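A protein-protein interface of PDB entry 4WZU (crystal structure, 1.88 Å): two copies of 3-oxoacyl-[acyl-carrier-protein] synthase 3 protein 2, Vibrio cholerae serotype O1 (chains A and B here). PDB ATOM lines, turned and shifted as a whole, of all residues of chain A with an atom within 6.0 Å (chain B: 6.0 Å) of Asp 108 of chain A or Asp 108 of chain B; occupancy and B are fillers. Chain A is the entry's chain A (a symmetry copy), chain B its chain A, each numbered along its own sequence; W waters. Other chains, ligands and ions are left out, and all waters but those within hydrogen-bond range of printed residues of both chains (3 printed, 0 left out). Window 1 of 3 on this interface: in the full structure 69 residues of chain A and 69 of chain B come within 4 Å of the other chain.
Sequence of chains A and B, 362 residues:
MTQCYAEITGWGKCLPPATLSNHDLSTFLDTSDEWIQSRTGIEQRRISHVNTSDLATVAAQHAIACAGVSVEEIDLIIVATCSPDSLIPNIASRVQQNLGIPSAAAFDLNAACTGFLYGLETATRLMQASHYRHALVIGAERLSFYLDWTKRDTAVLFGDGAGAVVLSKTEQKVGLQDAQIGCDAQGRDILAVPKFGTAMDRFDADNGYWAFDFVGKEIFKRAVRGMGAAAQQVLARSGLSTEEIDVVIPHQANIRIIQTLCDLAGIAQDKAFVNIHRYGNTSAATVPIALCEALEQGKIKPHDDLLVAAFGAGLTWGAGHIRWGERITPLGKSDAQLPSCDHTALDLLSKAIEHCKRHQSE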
ATOM      1  N   ILE A  77      35.073  -9.692   1.711  1.00  0.00           N
ATOM      2  CA  ILE A  77      35.253 -10.925   0.964  1.00  0.00           C
ATOM      3  C   ILE A  77      33.889 -11.404   0.485  1.00  0.00           C
ATOM      4  O   ILE A  77      32.989 -11.648   1.309  1.00  0.00           O
ATOM      5  CB  ILE A  77      35.849 -12.031   1.852  1.00  0.00           C
ATOM      6  CG1 ILE A  77      37.176 -11.589   2.467  1.00  0.00           C
ATOM      7  CG2 ILE A  77      36.032 -13.320   1.050  1.00  0.00           C
ATOM      8  CD1 ILE A  77      37.620 -12.459   3.649  1.00  0.00           C
ATOM      9  N   ILE A  78      33.727 -11.532  -0.830  1.00  0.00           N
ATOM     10  CA  ILE A  78      32.536 -12.090  -1.383  1.00  0.00           C
ATOM     11  C   ILE A  78      32.880 -13.373  -2.153  1.00  0.00           C
ATOM     12  O   ILE A  78      33.726 -13.340  -3.058  1.00  0.00           O
ATOM     13  CB  ILE A  78      31.847 -11.099  -2.316  1.00  0.00           C
ATOM     14  CG1 ILE A  78      31.484  -9.789  -1.577  1.00  0.00           C
ATOM     15  CG2 ILE A  78      30.604 -11.739  -2.889  1.00  0.00           C
ATOM     16  CD1 ILE A  78      30.733  -8.790  -2.419  1.00  0.00           C
ATOM     17  N   VAL A  79      32.207 -14.483  -1.842  1.00  0.00           N
ATOM     18  CA  VAL A  79      32.339 -15.673  -2.670  1.00  0.00           C
ATOM     19  C   VAL A  79      31.039 -15.862  -3.390  1.00  0.00           C
ATOM     20  O   VAL A  79      29.991 -16.113  -2.745  1.00  0.00           O
ATOM     21  CB  VAL A  79      32.679 -16.957  -1.889  1.00  0.00           C
ATOM     22  CG1 VAL A  79      32.775 -18.148  -2.843  1.00  0.00           C
ATOM     23  CG2 VAL A  79      33.979 -16.773  -1.108  1.00  0.00           C
ATOM     24  N   ALA A  80      31.096 -15.711  -4.717  1.00  0.00           N
ATOM     25  CA  ALA A  80      29.973 -15.990  -5.566  1.00  0.00           C
ATOM     26  C   ALA A  80      30.010 -17.481  -5.858  1.00  0.00           C
ATOM     27  O   ALA A  80      30.963 -17.961  -6.448  1.00  0.00           O
ATOM     28  CB  ALA A  80      30.044 -15.191  -6.856  1.00  0.00           C
ATOM     29  N   THR A  81      29.015 -18.217  -5.378  1.00  0.00           N
ATOM     30  CA  THR A  81      28.932 -19.647  -5.653  1.00  0.00           C
ATOM     31  C   THR A  81      27.496 -20.113  -5.561  1.00  0.00           C
ATOM     32  O   THR A  81      26.661 -19.477  -4.875  1.00  0.00           O
ATOM     33  CB  THR A  81      29.844 -20.426  -4.688  1.00  0.00           C
ATOM     34  OG1 THR A  81      29.891 -21.820  -5.038  1.00  0.00           O
ATOM     35  CG2 THR A  81      29.411 -20.265  -3.251  1.00  0.00           C
ATOM     36  N   PRO A  84      28.407 -24.226  -2.560  1.00  0.00           N
ATOM     37  CA  PRO A  84      29.207 -24.083  -1.334  1.00  0.00           C
ATOM     38  C   PRO A  84      29.382 -25.400  -0.591  1.00  0.00           C
ATOM     39  O   PRO A  84      28.437 -26.153  -0.512  1.00  0.00           O
ATOM     40  CB  PRO A  84      28.367 -23.110  -0.500  1.00  0.00           C
ATOM     41  CG  PRO A  84      26.965 -23.375  -0.925  1.00  0.00           C
ATOM     42  CD  PRO A  84      27.068 -23.622  -2.411  1.00  0.00           C
ATOM     43  N   SER A  86      29.337 -25.787   2.465  1.00  0.00           N
ATOM     44  CA  SER A  86      28.380 -25.734   3.560  1.00  0.00           C
ATOM     45  C   SER A  86      27.544 -24.457   3.473  1.00  0.00           C
ATOM     46  O   SER A  86      27.915 -23.484   2.781  1.00  0.00           O
ATOM     47  CB  SER A  86      29.117 -25.766   4.907  1.00  0.00           C
ATOM     48  OG  SER A  86      29.833 -24.553   5.165  1.00  0.00           O
ATOM     49  N   PRO A  89      28.728 -22.759   8.385  1.00  0.00           N
ATOM     50  CA  PRO A  89      28.715 -21.347   8.003  1.00  0.00           C
ATOM     51  C   PRO A  89      28.892 -21.178   6.495  1.00  0.00           C
ATOM     52  O   PRO A  89      28.971 -22.176   5.764  1.00  0.00           O
ATOM     53  CB  PRO A  89      29.965 -20.784   8.730  1.00  0.00           C
ATOM     54  CG  PRO A  89      30.644 -21.959   9.372  1.00  0.00           C
ATOM     55  CD  PRO A  89      30.081 -23.194   8.730  1.00  0.00           C
ATOM     56  N   ASN A  90      28.987 -19.928   6.042  1.00  0.00           N
ATOM     57  CA  ASN A  90      29.257 -19.626   4.625  1.00  0.00           C
ATOM     58  C   ASN A  90      30.699 -20.008   4.279  1.00  0.00           C
ATOM     59  O   ASN A  90      31.505 -20.230   5.194  1.00  0.00           O
ATOM     60  CB  ASN A  90      28.945 -18.145   4.309  1.00  0.00           C
ATOM     61  CG  ASN A  90      29.867 -17.143   5.021  1.00  0.00           C
ATOM     62  OD1 ASN A  90      31.017 -17.430   5.354  1.00  0.00           O
ATOM     63  ND2 ASN A  90      29.339 -15.965   5.280  1.00  0.00           N
ATOM     64  N   ILE A  91      31.056 -20.094   2.998  1.00  0.00           N
ATOM     65  CA  ILE A  91      32.436 -20.430   2.668  1.00  0.00           C
ATOM     66  C   ILE A  91      33.335 -19.217   2.485  1.00  0.00           C
ATOM     67  O   ILE A  91      34.547 -19.351   2.514  1.00  0.00           O
ATOM     68  CB  ILE A  91      32.566 -21.453   1.508  1.00  0.00           C
ATOM     69  CG1 ILE A  91      32.026 -20.927   0.187  1.00  0.00           C
ATOM     70  CG2 ILE A  91      31.840 -22.744   1.861  1.00  0.00           C
ATOM     71  CD1 ILE A  91      32.546 -21.702  -1.017  1.00  0.00           C
ATOM     72  N   ALA A  92      32.769 -18.026   2.321  1.00  0.00           N
ATOM     73  CA  ALA A  92      33.596 -16.835   2.401  1.00  0.00           C
ATOM     74  C   ALA A  92      34.399 -16.821   3.704  1.00  0.00           C
ATOM     75  O   ALA A  92      35.590 -16.510   3.675  1.00  0.00           O
ATOM     76  CB  ALA A  92      32.764 -15.581   2.251  1.00  0.00           C
ATOM     77  N   SER A  93      33.764 -17.162   4.828  1.00  0.00           N
ATOM     78  CA  SER A  93      34.463 -17.244   6.101  1.00  0.00           C
ATOM     79  C   SER A  93      35.548 -18.330   6.140  1.00  0.00           C
ATOM     80  O   SER A  93      36.517 -18.192   6.861  1.00  0.00           O
ATOM     81  CB  SER A  93      33.480 -17.419   7.273  1.00  0.00           C
ATOM     82  OG  SER A  93      32.766 -18.661   7.200  1.00  0.00           O
ATOM     83  N   ALA A 106      32.418 -10.968   5.381  1.00  0.00           N
ATOM     84  CA  ALA A 106      32.528 -12.145   4.537  1.00  0.00           C
ATOM     85  C   ALA A 106      31.162 -12.754   4.281  1.00  0.00           C
ATOM     86  O   ALA A 106      30.473 -13.213   5.225  1.00  0.00           O
ATOM     87  CB  ALA A 106      33.459 -13.166   5.197  1.00  0.00           C
ATOM     88  N   PHE A 107      30.769 -12.780   3.011  1.00  0.00           N
ATOM     89  CA  PHE A 107      29.511 -13.428   2.644  1.00  0.00           C
ATOM     90  C   PHE A 107      29.520 -14.179   1.337  1.00  0.00           C
ATOM     91  O   PHE A 107      30.349 -13.910   0.480  1.00  0.00           O
ATOM     92  CB  PHE A 107      28.337 -12.462   2.754  1.00  0.00           C
ATOM     93  CG  PHE A 107      28.308 -11.367   1.730  1.00  0.00           C
ATOM     94  CD1 PHE A 107      27.624 -11.557   0.526  1.00  0.00           C
ATOM     95  CD2 PHE A 107      28.839 -10.119   2.001  1.00  0.00           C
ATOM     96  CE1 PHE A 107      27.553 -10.543  -0.397  1.00  0.00           C
ATOM     97  CE2 PHE A 107      28.746  -9.097   1.080  1.00  0.00           C
ATOM     98  CZ  PHE A 107      28.109  -9.307  -0.112  1.00  0.00           C
ATOM     99  N   ASP A 108      28.642 -15.188   1.249  1.00  0.00           N
ATOM    100  CA  ASP A 108      28.405 -15.908   0.004  1.00  0.00           C
ATOM    101  C   ASP A 108      27.248 -15.235  -0.724  1.00  0.00           C
ATOM    102  O   ASP A 108      26.253 -14.828  -0.122  1.00  0.00           O
ATOM    103  CB  ASP A 108      28.101 -17.415   0.192  1.00  0.00           C
ATOM    104  CG  ASP A 108      29.255 -18.188   0.850  1.00  0.00           C
ATOM    105  OD1 ASP A 108      30.360 -17.594   1.031  1.00  0.00           O
ATOM    106  OD2 ASP A 108      29.049 -19.391   1.233  1.00  0.00           O
ATOM    107  N   LEU A 109      27.406 -15.099  -2.033  1.00  0.00           N
ATOM    108  CA  LEU A 109      26.421 -14.488  -2.865  1.00  0.00           C
ATOM    109  C   LEU A 109      26.034 -15.527  -3.899  1.00  0.00           C
ATOM    110  O   LEU A 109      26.896 -16.043  -4.615  1.00  0.00           O
ATOM    111  CB  LEU A 109      27.030 -13.229  -3.538  1.00  0.00           C
ATOM    112  CG  LEU A 109      26.078 -12.335  -4.340  1.00  0.00           C
ATOM    113  CD1 LEU A 109      26.644 -10.935  -4.519  1.00  0.00           C
ATOM    114  CD2 LEU A 109      25.778 -12.940  -5.694  1.00  0.00           C
ATOM    115  N   ASN A 110      24.740 -15.819  -4.008  1.00  0.00           N
ATOM    116  CA  ASN A 110      24.251 -16.762  -4.999  1.00  0.00           C
ATOM    117  C   ASN A 110      23.347 -16.069  -6.029  1.00  0.00           C
ATOM    118  O   ASN A 110      22.212 -15.721  -5.747  1.00  0.00           O
ATOM    119  CB  ASN A 110      23.506 -17.918  -4.325  1.00  0.00           C
ATOM    120  CG  ASN A 110      22.999 -18.945  -5.325  1.00  0.00           C
ATOM    121  OD1 ASN A 110      23.343 -18.909  -6.506  1.00  0.00           O
ATOM    122  ND2 ASN A 110      22.140 -19.831  -4.865  1.00  0.00           N
ATOM    123  N   ALA A 111      23.907 -15.850  -7.214  1.00  0.00           N
ATOM    124  CA  ALA A 111      23.144 -15.506  -8.427  1.00  0.00           C
ATOM    125  C   ALA A 111      23.533 -16.396  -9.620  1.00  0.00           C
ATOM    126  O   ALA A 111      23.558 -15.945 -10.776  1.00  0.00           O
ATOM    127  CB  ALA A 111      23.367 -14.040  -8.750  1.00  0.00           C
ATOM    128  N   ILE B  77      16.412  -7.214  -5.165  1.00  0.00           N
ATOM    129  CA  ILE B  77      15.862  -8.142  -4.190  1.00  0.00           C
ATOM    130  C   ILE B  77      17.007  -8.935  -3.577  1.00  0.00           C
ATOM    131  O   ILE B  77      17.747  -9.624  -4.304  1.00  0.00           O
ATOM    132  CB  ILE B  77      14.904  -9.145  -4.856  1.00  0.00           C
ATOM    133  CG1 ILE B  77      13.776  -8.424  -5.594  1.00  0.00           C
ATOM    134  CG2 ILE B  77      14.334 -10.111  -3.817  1.00  0.00           C
ATOM    135  CD1 ILE B  77      13.029  -9.319  -6.590  1.00  0.00           C
ATOM    136  N   ILE B  78      17.164  -8.842  -2.258  1.00  0.00           N
ATOM    137  CA  ILE B  78      18.122  -9.637  -1.563  1.00  0.00           C
ATOM    138  C   ILE B  78      17.402 -10.551  -0.562  1.00  0.00           C
ATOM    139  O   ILE B  78      16.645 -10.058   0.288  1.00  0.00           O
ATOM    140  CB  ILE B  78      19.131  -8.761  -0.827  1.00  0.00           C
ATOM    141  CG1 ILE B  78      19.880  -7.823  -1.803  1.00  0.00           C
ATOM    142  CG2 ILE B  78      20.113  -9.645  -0.093  1.00  0.00           C
ATOM    143  CD1 ILE B  78      20.947  -6.979  -1.154  1.00  0.00           C
ATOM    144  N   VAL B  79      17.659 -11.859  -0.618  1.00  0.00           N
ATOM    145  CA  VAL B  79      17.171 -12.746   0.427  1.00  0.00           C
ATOM    146  C   VAL B  79      18.361 -13.203   1.216  1.00  0.00           C
ATOM    147  O   VAL B  79      19.245 -13.910   0.672  1.00  0.00           O
ATOM    148  CB  VAL B  79      16.400 -13.976  -0.089  1.00  0.00           C
ATOM    149  CG1 VAL B  79      15.950 -14.849   1.083  1.00  0.00           C
ATOM    150  CG2 VAL B  79      15.207 -13.535  -0.935  1.00  0.00           C
ATOM    151  N   ALA B  80      18.403 -12.776   2.482  1.00  0.00           N
ATOM    152  CA  ALA B  80      19.400 -13.233   3.408  1.00  0.00           C
ATOM    153  C   ALA B  80      18.883 -14.536   3.994  1.00  0.00           C
ATOM    154  O   ALA B  80      17.847 -14.545   4.635  1.00  0.00           O
ATOM    155  CB  ALA B  80      19.641 -12.211   4.507  1.00  0.00           C
ATOM    156  N   THR B  81      19.563 -15.639   3.708  1.00  0.00           N
ATOM    157  CA  THR B  81      19.179 -16.930   4.270  1.00  0.00           C
ATOM    158  C   THR B  81      20.377 -17.851   4.323  1.00  0.00           C
ATOM    159  O   THR B  81      21.351 -17.679   3.552  1.00  0.00           O
ATOM    160  CB  THR B  81      18.028 -17.543   3.451  1.00  0.00           C
ATOM    161  OG1 THR B  81      17.536 -18.742   4.074  1.00  0.00           O
ATOM    162  CG2 THR B  81      18.441 -17.828   2.027  1.00  0.00           C
ATOM    163  N   PRO B  84      18.057 -21.951   2.187  1.00  0.00           N
ATOM    164  CA  PRO B  84      17.308 -21.804   0.930  1.00  0.00           C
ATOM    165  C   PRO B  84      16.683 -23.111   0.463  1.00  0.00           C
ATOM    166  O   PRO B  84      17.323 -24.133   0.571  1.00  0.00           O
ATOM    167  CB  PRO B  84      18.391 -21.352  -0.054  1.00  0.00           C
ATOM    168  CG  PRO B  84      19.642 -21.973   0.464  1.00  0.00           C
ATOM    169  CD  PRO B  84      19.515 -21.866   1.965  1.00  0.00           C
ATOM    170  N   SER B  86      16.491 -24.100  -2.447  1.00  0.00           N
ATOM    171  CA  SER B  86      17.373 -24.588  -3.497  1.00  0.00           C
ATOM    172  C   SER B  86      18.586 -23.669  -3.641  1.00  0.00           C
ATOM    173  O   SER B  86      18.581 -22.509  -3.174  1.00  0.00           O
ATOM    174  CB  SER B  86      16.620 -24.648  -4.835  1.00  0.00           C
ATOM    175  OG  SER B  86      16.336 -23.346  -5.358  1.00  0.00           O
ATOM    176  N   PRO B  89      17.858 -22.707  -8.834  1.00  0.00           N
ATOM    177  CA  PRO B  89      18.349 -21.332  -8.745  1.00  0.00           C
ATOM    178  C   PRO B  89      18.291 -20.813  -7.309  1.00  0.00           C
ATOM    179  O   PRO B  89      17.913 -21.559  -6.394  1.00  0.00           O
ATOM    180  CB  PRO B  89      17.330 -20.548  -9.613  1.00  0.00           C
ATOM    181  CG  PRO B  89      16.280 -21.536 -10.028  1.00  0.00           C
ATOM    182  CD  PRO B  89      16.427 -22.732  -9.129  1.00  0.00           C
ATOM    183  N   ASN B  90      18.629 -19.536  -7.122  1.00  0.00           N
ATOM    184  CA  ASN B  90      18.523 -18.883  -5.805  1.00  0.00           C
ATOM    185  C   ASN B  90      17.048 -18.689  -5.440  1.00  0.00           C
ATOM    186  O   ASN B  90      16.183 -18.814  -6.318  1.00  0.00           O
ATOM    187  CB  ASN B  90      19.316 -17.556  -5.785  1.00  0.00           C
ATOM    188  CG  ASN B  90      18.752 -16.472  -6.716  1.00  0.00           C
ATOM    189  OD1 ASN B  90      17.561 -16.424  -7.024  1.00  0.00           O
ATOM    190  ND2 ASN B  90      19.629 -15.612  -7.190  1.00  0.00           N
ATOM    191  N   ILE B  91      16.728 -18.392  -4.180  1.00  0.00           N
ATOM    192  CA  ILE B  91      15.327 -18.180  -3.837  1.00  0.00           C
ATOM    193  C   ILE B  91      14.884 -16.728  -3.935  1.00  0.00           C
ATOM    194  O   ILE B  91      13.696 -16.458  -3.979  1.00  0.00           O
ATOM    195  CB  ILE B  91      14.906 -18.846  -2.500  1.00  0.00           C
ATOM    196  CG1 ILE B  91      15.635 -18.272  -1.294  1.00  0.00           C
ATOM    197  CG2 ILE B  91      15.154 -20.347  -2.560  1.00  0.00           C
ATOM    198  CD1 ILE B  91      14.931 -18.571   0.023  1.00  0.00           C
ATOM    199  N   ALA B  92      15.816 -15.783  -3.996  1.00  0.00           N
ATOM    200  CA  ALA B  92      15.426 -14.429  -4.344  1.00  0.00           C
ATOM    201  C   ALA B  92      14.628 -14.414  -5.650  1.00  0.00           C
ATOM    202  O   ALA B  92      13.609 -13.729  -5.726  1.00  0.00           O
ATOM    203  CB  ALA B  92      16.630 -13.516  -4.422  1.00  0.00           C
ATOM    204  N   SER B  93      15.077 -15.165  -6.659  1.00  0.00           N
ATOM    205  CA  SER B  93      14.345 -15.269  -7.912  1.00  0.00           C
ATOM    206  C   SER B  93      12.962 -15.920  -7.769  1.00  0.00           C
ATOM    207  O   SER B  93      12.068 -15.619  -8.536  1.00  0.00           O
ATOM    208  CB  SER B  93      15.175 -15.990  -8.990  1.00  0.00           C
ATOM    209  OG  SER B  93      15.441 -17.356  -8.642  1.00  0.00           O
ATOM    210  N   ALA B 106      18.368 -10.009  -8.407  1.00  0.00           N
ATOM    211  CA  ALA B 106      17.906 -10.888  -7.346  1.00  0.00           C
ATOM    212  C   ALA B 106      19.003 -11.848  -6.925  1.00  0.00           C
ATOM    213  O   ALA B 106      19.470 -12.689  -7.732  1.00  0.00           O
ATOM    214  CB  ALA B 106      16.669 -11.656  -7.818  1.00  0.00           C
ATOM    215  N   PHE B 107      19.410 -11.745  -5.662  1.00  0.00           N
ATOM    216  CA  PHE B 107      20.395 -12.683  -5.129  1.00  0.00           C
ATOM    217  C   PHE B 107      20.185 -13.107  -3.699  1.00  0.00           C
ATOM    218  O   PHE B 107      19.521 -12.413  -2.943  1.00  0.00           O
ATOM    219  CB  PHE B 107      21.818 -12.201  -5.392  1.00  0.00           C
ATOM    220  CG  PHE B 107      22.242 -10.994  -4.610  1.00  0.00           C
ATOM    221  CD1 PHE B 107      22.866 -11.151  -3.370  1.00  0.00           C
ATOM    222  CD2 PHE B 107      22.142  -9.722  -5.146  1.00  0.00           C
ATOM    223  CE1 PHE B 107      23.299 -10.053  -2.668  1.00  0.00           C
ATOM    224  CE2 PHE B 107      22.600  -8.625  -4.448  1.00  0.00           C
ATOM    225  CZ  PHE B 107      23.172  -8.787  -3.217  1.00  0.00           C
ATOM    226  N   ASP B 108      20.683 -14.310  -3.378  1.00  0.00           N
ATOM    227  CA  ASP B 108      20.713 -14.800  -2.006  1.00  0.00           C
ATOM    228  C   ASP B 108      22.052 -14.414  -1.389  1.00  0.00           C
ATOM    229  O   ASP B 108      23.103 -14.488  -2.026  1.00  0.00           O
ATOM    230  CB  ASP B 108      20.496 -16.328  -1.874  1.00  0.00           C
ATOM    231  CG  ASP B 108      19.129 -16.793  -2.401  1.00  0.00           C
ATOM    232  OD1 ASP B 108      18.277 -15.918  -2.737  1.00  0.00           O
ATOM    233  OD2 ASP B 108      18.914 -18.048  -2.526  1.00  0.00           O
ATOM    234  N   LEU B 109      21.992 -13.971  -0.141  1.00  0.00           N
ATOM    235  CA  LEU B 109      23.152 -13.564   0.584  1.00  0.00           C
ATOM    236  C   LEU B 109      23.210 -14.441   1.819  1.00  0.00           C
ATOM    237  O   LEU B 109      22.252 -14.488   2.595  1.00  0.00           O
ATOM    238  CB  LEU B 109      23.016 -12.067   0.967  1.00  0.00           C
ATOM    239  CG  LEU B 109      24.236 -11.394   1.604  1.00  0.00           C
ATOM    240  CD1 LEU B 109      24.170  -9.880   1.477  1.00  0.00           C
ATOM    241  CD2 LEU B 109      24.368 -11.777   3.062  1.00  0.00           C
ATOM    242  N   ASN B 110      24.339 -15.114   2.030  1.00  0.00           N
ATOM    243  CA  ASN B 110      24.524 -15.945   3.208  1.00  0.00           C
ATOM    244  C   ASN B 110      25.641 -15.395   4.108  1.00  0.00           C
ATOM    245  O   ASN B 110      26.817 -15.506   3.800  1.00  0.00           O
ATOM    246  CB  ASN B 110      24.822 -17.393   2.808  1.00  0.00           C
ATOM    247  CG  ASN B 110      24.997 -18.305   4.012  1.00  0.00           C
ATOM    248  OD1 ASN B 110      24.725 -17.919   5.149  1.00  0.00           O
ATOM    249  ND2 ASN B 110      25.499 -19.498   3.771  1.00  0.00           N
ATOM    250  N   ALA B 111      25.226 -14.769   5.204  1.00  0.00           N
ATOM    251  CA  ALA B 111      26.101 -14.458   6.348  1.00  0.00           C
ATOM    252  C   ALA B 111      25.483 -14.909   7.682  1.00  0.00           C
ATOM    253  O   ALA B 111      25.648 -14.252   8.721  1.00  0.00           O
ATOM    254  CB  ALA B 111      26.386 -12.968   6.359  1.00  0.00           C
HETATM  255  O   HOH W   1      26.902 -20.804   1.640  1.00  0.00           O
HETATM  256  O   HOH W   2      24.240 -17.212  -0.805  1.00  0.00           O
HETATM  257  O   HOH W   3      20.460 -20.142  -2.564  1.00  0.00           O
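The side-chain amide nitrogen (ND2) of Asn 90 of chain B is in hydrogen-bond range of the backbone carbonyl oxygen (O) of Asn 110 of chain A, 3.0 Å away.
The backbone carbonyl oxygen (O) of Asp 108 of chain B sits at hydrogen-bond distance from the backbone NH (N) of Asn 110 of chain A (2.9 Å).
O of Asn 110 of chain B is in hydrogen-bond range of ND2 of Asn 90 of chain A.
N of Asn 110 of chain B is in hydrogen-bond range of O of Asp 108 of chain A, 2.9 Å away.
Ala 106 of chain A touches none of the printed residues of chain B.
Printed residues of chain B within 4 Å of Phe 107 of chain A: Leu 109 (3.6 Å) and Asn 110 (3.6 Å).
Of chain B, only Asp 108 (3.7 Å), Leu 109 (3.4 Å) and Asn 110 (2.9 Å) come within 4 Å of Asp 108 of chain A.
Of the printed residues of chain B, Asn 110 of chain A touches Asn 90 (3.0 Å), Phe 107 (3.6 Å) and Asp 108 (2.9 Å).
Of the printed residues of chain B, Ala 111 of chain A touches Asn 90.
Ser 93 of chain B touches none of the printed residues of chain A.
Asp 108 of chain B touches just these residues of chain A: Asp 108 (3.7 Å), Leu 109 (3.4 Å) and Asn 110 (2.9 Å).
Of the printed residues of chain A, Ala 111 of chain B touches Asn 90.
The nearest residue of chain B that does not touch Asp 108 of chain A is Ala 111 of chain B (5.2 Å).
The nearest residue of chain A that does not touch Asp 108 of chain B is Ala 111 of chain A (5.2 Å).
Among the printed residues, pairs that only touch across the chains: Asn 90 of chain A with Ala 111 of chain B, Phe 107 of chain A with Leu 109 of chain B, Phe 107 of chain A with Asn 110 of chain B, Asp 108 of chain A with Asp 108 of chain B, Asp 108 of chain A with Leu 109 of chain B, Leu 109 of chain A with Phe 107 of chain B, Leu 109 of chain A with Asp 108 of chain B, Asn 110 of chain A with Phe 107 of chain B and Ala 111 of chain A with Asn 90 of chain B.
N of Phe 107 of chain B sits at hydrogen-bond distance from O of Ile 77 of chain B (3.0 Å).
The backbone carbonyl oxygen of Leu 109 of chain B sits at hydrogen-bond distance from the backbone NH of Thr 81 of chain B (3.1 Å).
OD1 of Asn 90 of chain B sits at hydrogen-bond distance from N of Ser 93 of chain B (2.8 Å).
The side-chain carboxylate (OD2) of Asp 108 of chain B is in hydrogen-bond range of the backbone NH (N) of Ile 91 of chain B (2.8 Å).
The backbone NH (N) of Thr 81 of chain A lies within hydrogen-bond range of the backbone carbonyl oxygen (O) of Leu 109 of chain A, at 3.1 Å.
OD1 of Asp 108 of chain A sits at hydrogen-bond distance from N of Ala 92 of chain A (2.8 Å).
Asn 90 of chain A touches Ala 111 of chain B, and with the chains exchanged Ala 111 of chain A touches Asn 90 of chain B.
Phe 107 of chain A touches Asn 110 of chain B, and with the chains exchanged Asn 110 of chain A touches Phe 107 of chain B.
Asp 108 of chain B touches its own counterpart, Asp 108 of chain A.
Asp 108 of chain A touches Leu 109 of chain B, and with the chains exchanged Leu 109 of chain A touches Asp 108 of chain B.
Of the 13 pairs that touch across the chains among the printed residues, 13 have their exchanged pair printed and touching as well.
Water W1 lies within hydrogen-bond range of OD2 of Asp 108 of chain A (2.6 Å), ND2 of Asn 110 of chain B (2.9 Å) and O of Ser 86 of chain A (3.1 Å).
Water W3 lies within hydrogen-bond range of OD2 of Asp 108 of chain B (2.6 Å), ND2 of Asn 110 of chain A (2.9 Å) and O of Ser 86 of chain B (3.1 Å).
Water W2 lies within hydrogen-bond range of the backbone carbonyl oxygen (O) of Asp 108 of chain A (3.2 Å) and the backbone carbonyl oxygen (O) of Asp 108 of chain B (3.2 Å).
Of the 18 printed residues of chain A, 6 touch a printed residue of chain B.
Hydrophobic or aromatic side chains of chain A that line the printed part of chain B: Phe 107 and Leu 109.
Among the printed residues, no Asp or Glu carboxylate lies within 4 Å of a Lys or Arg side-chain nitrogen of the other chain.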
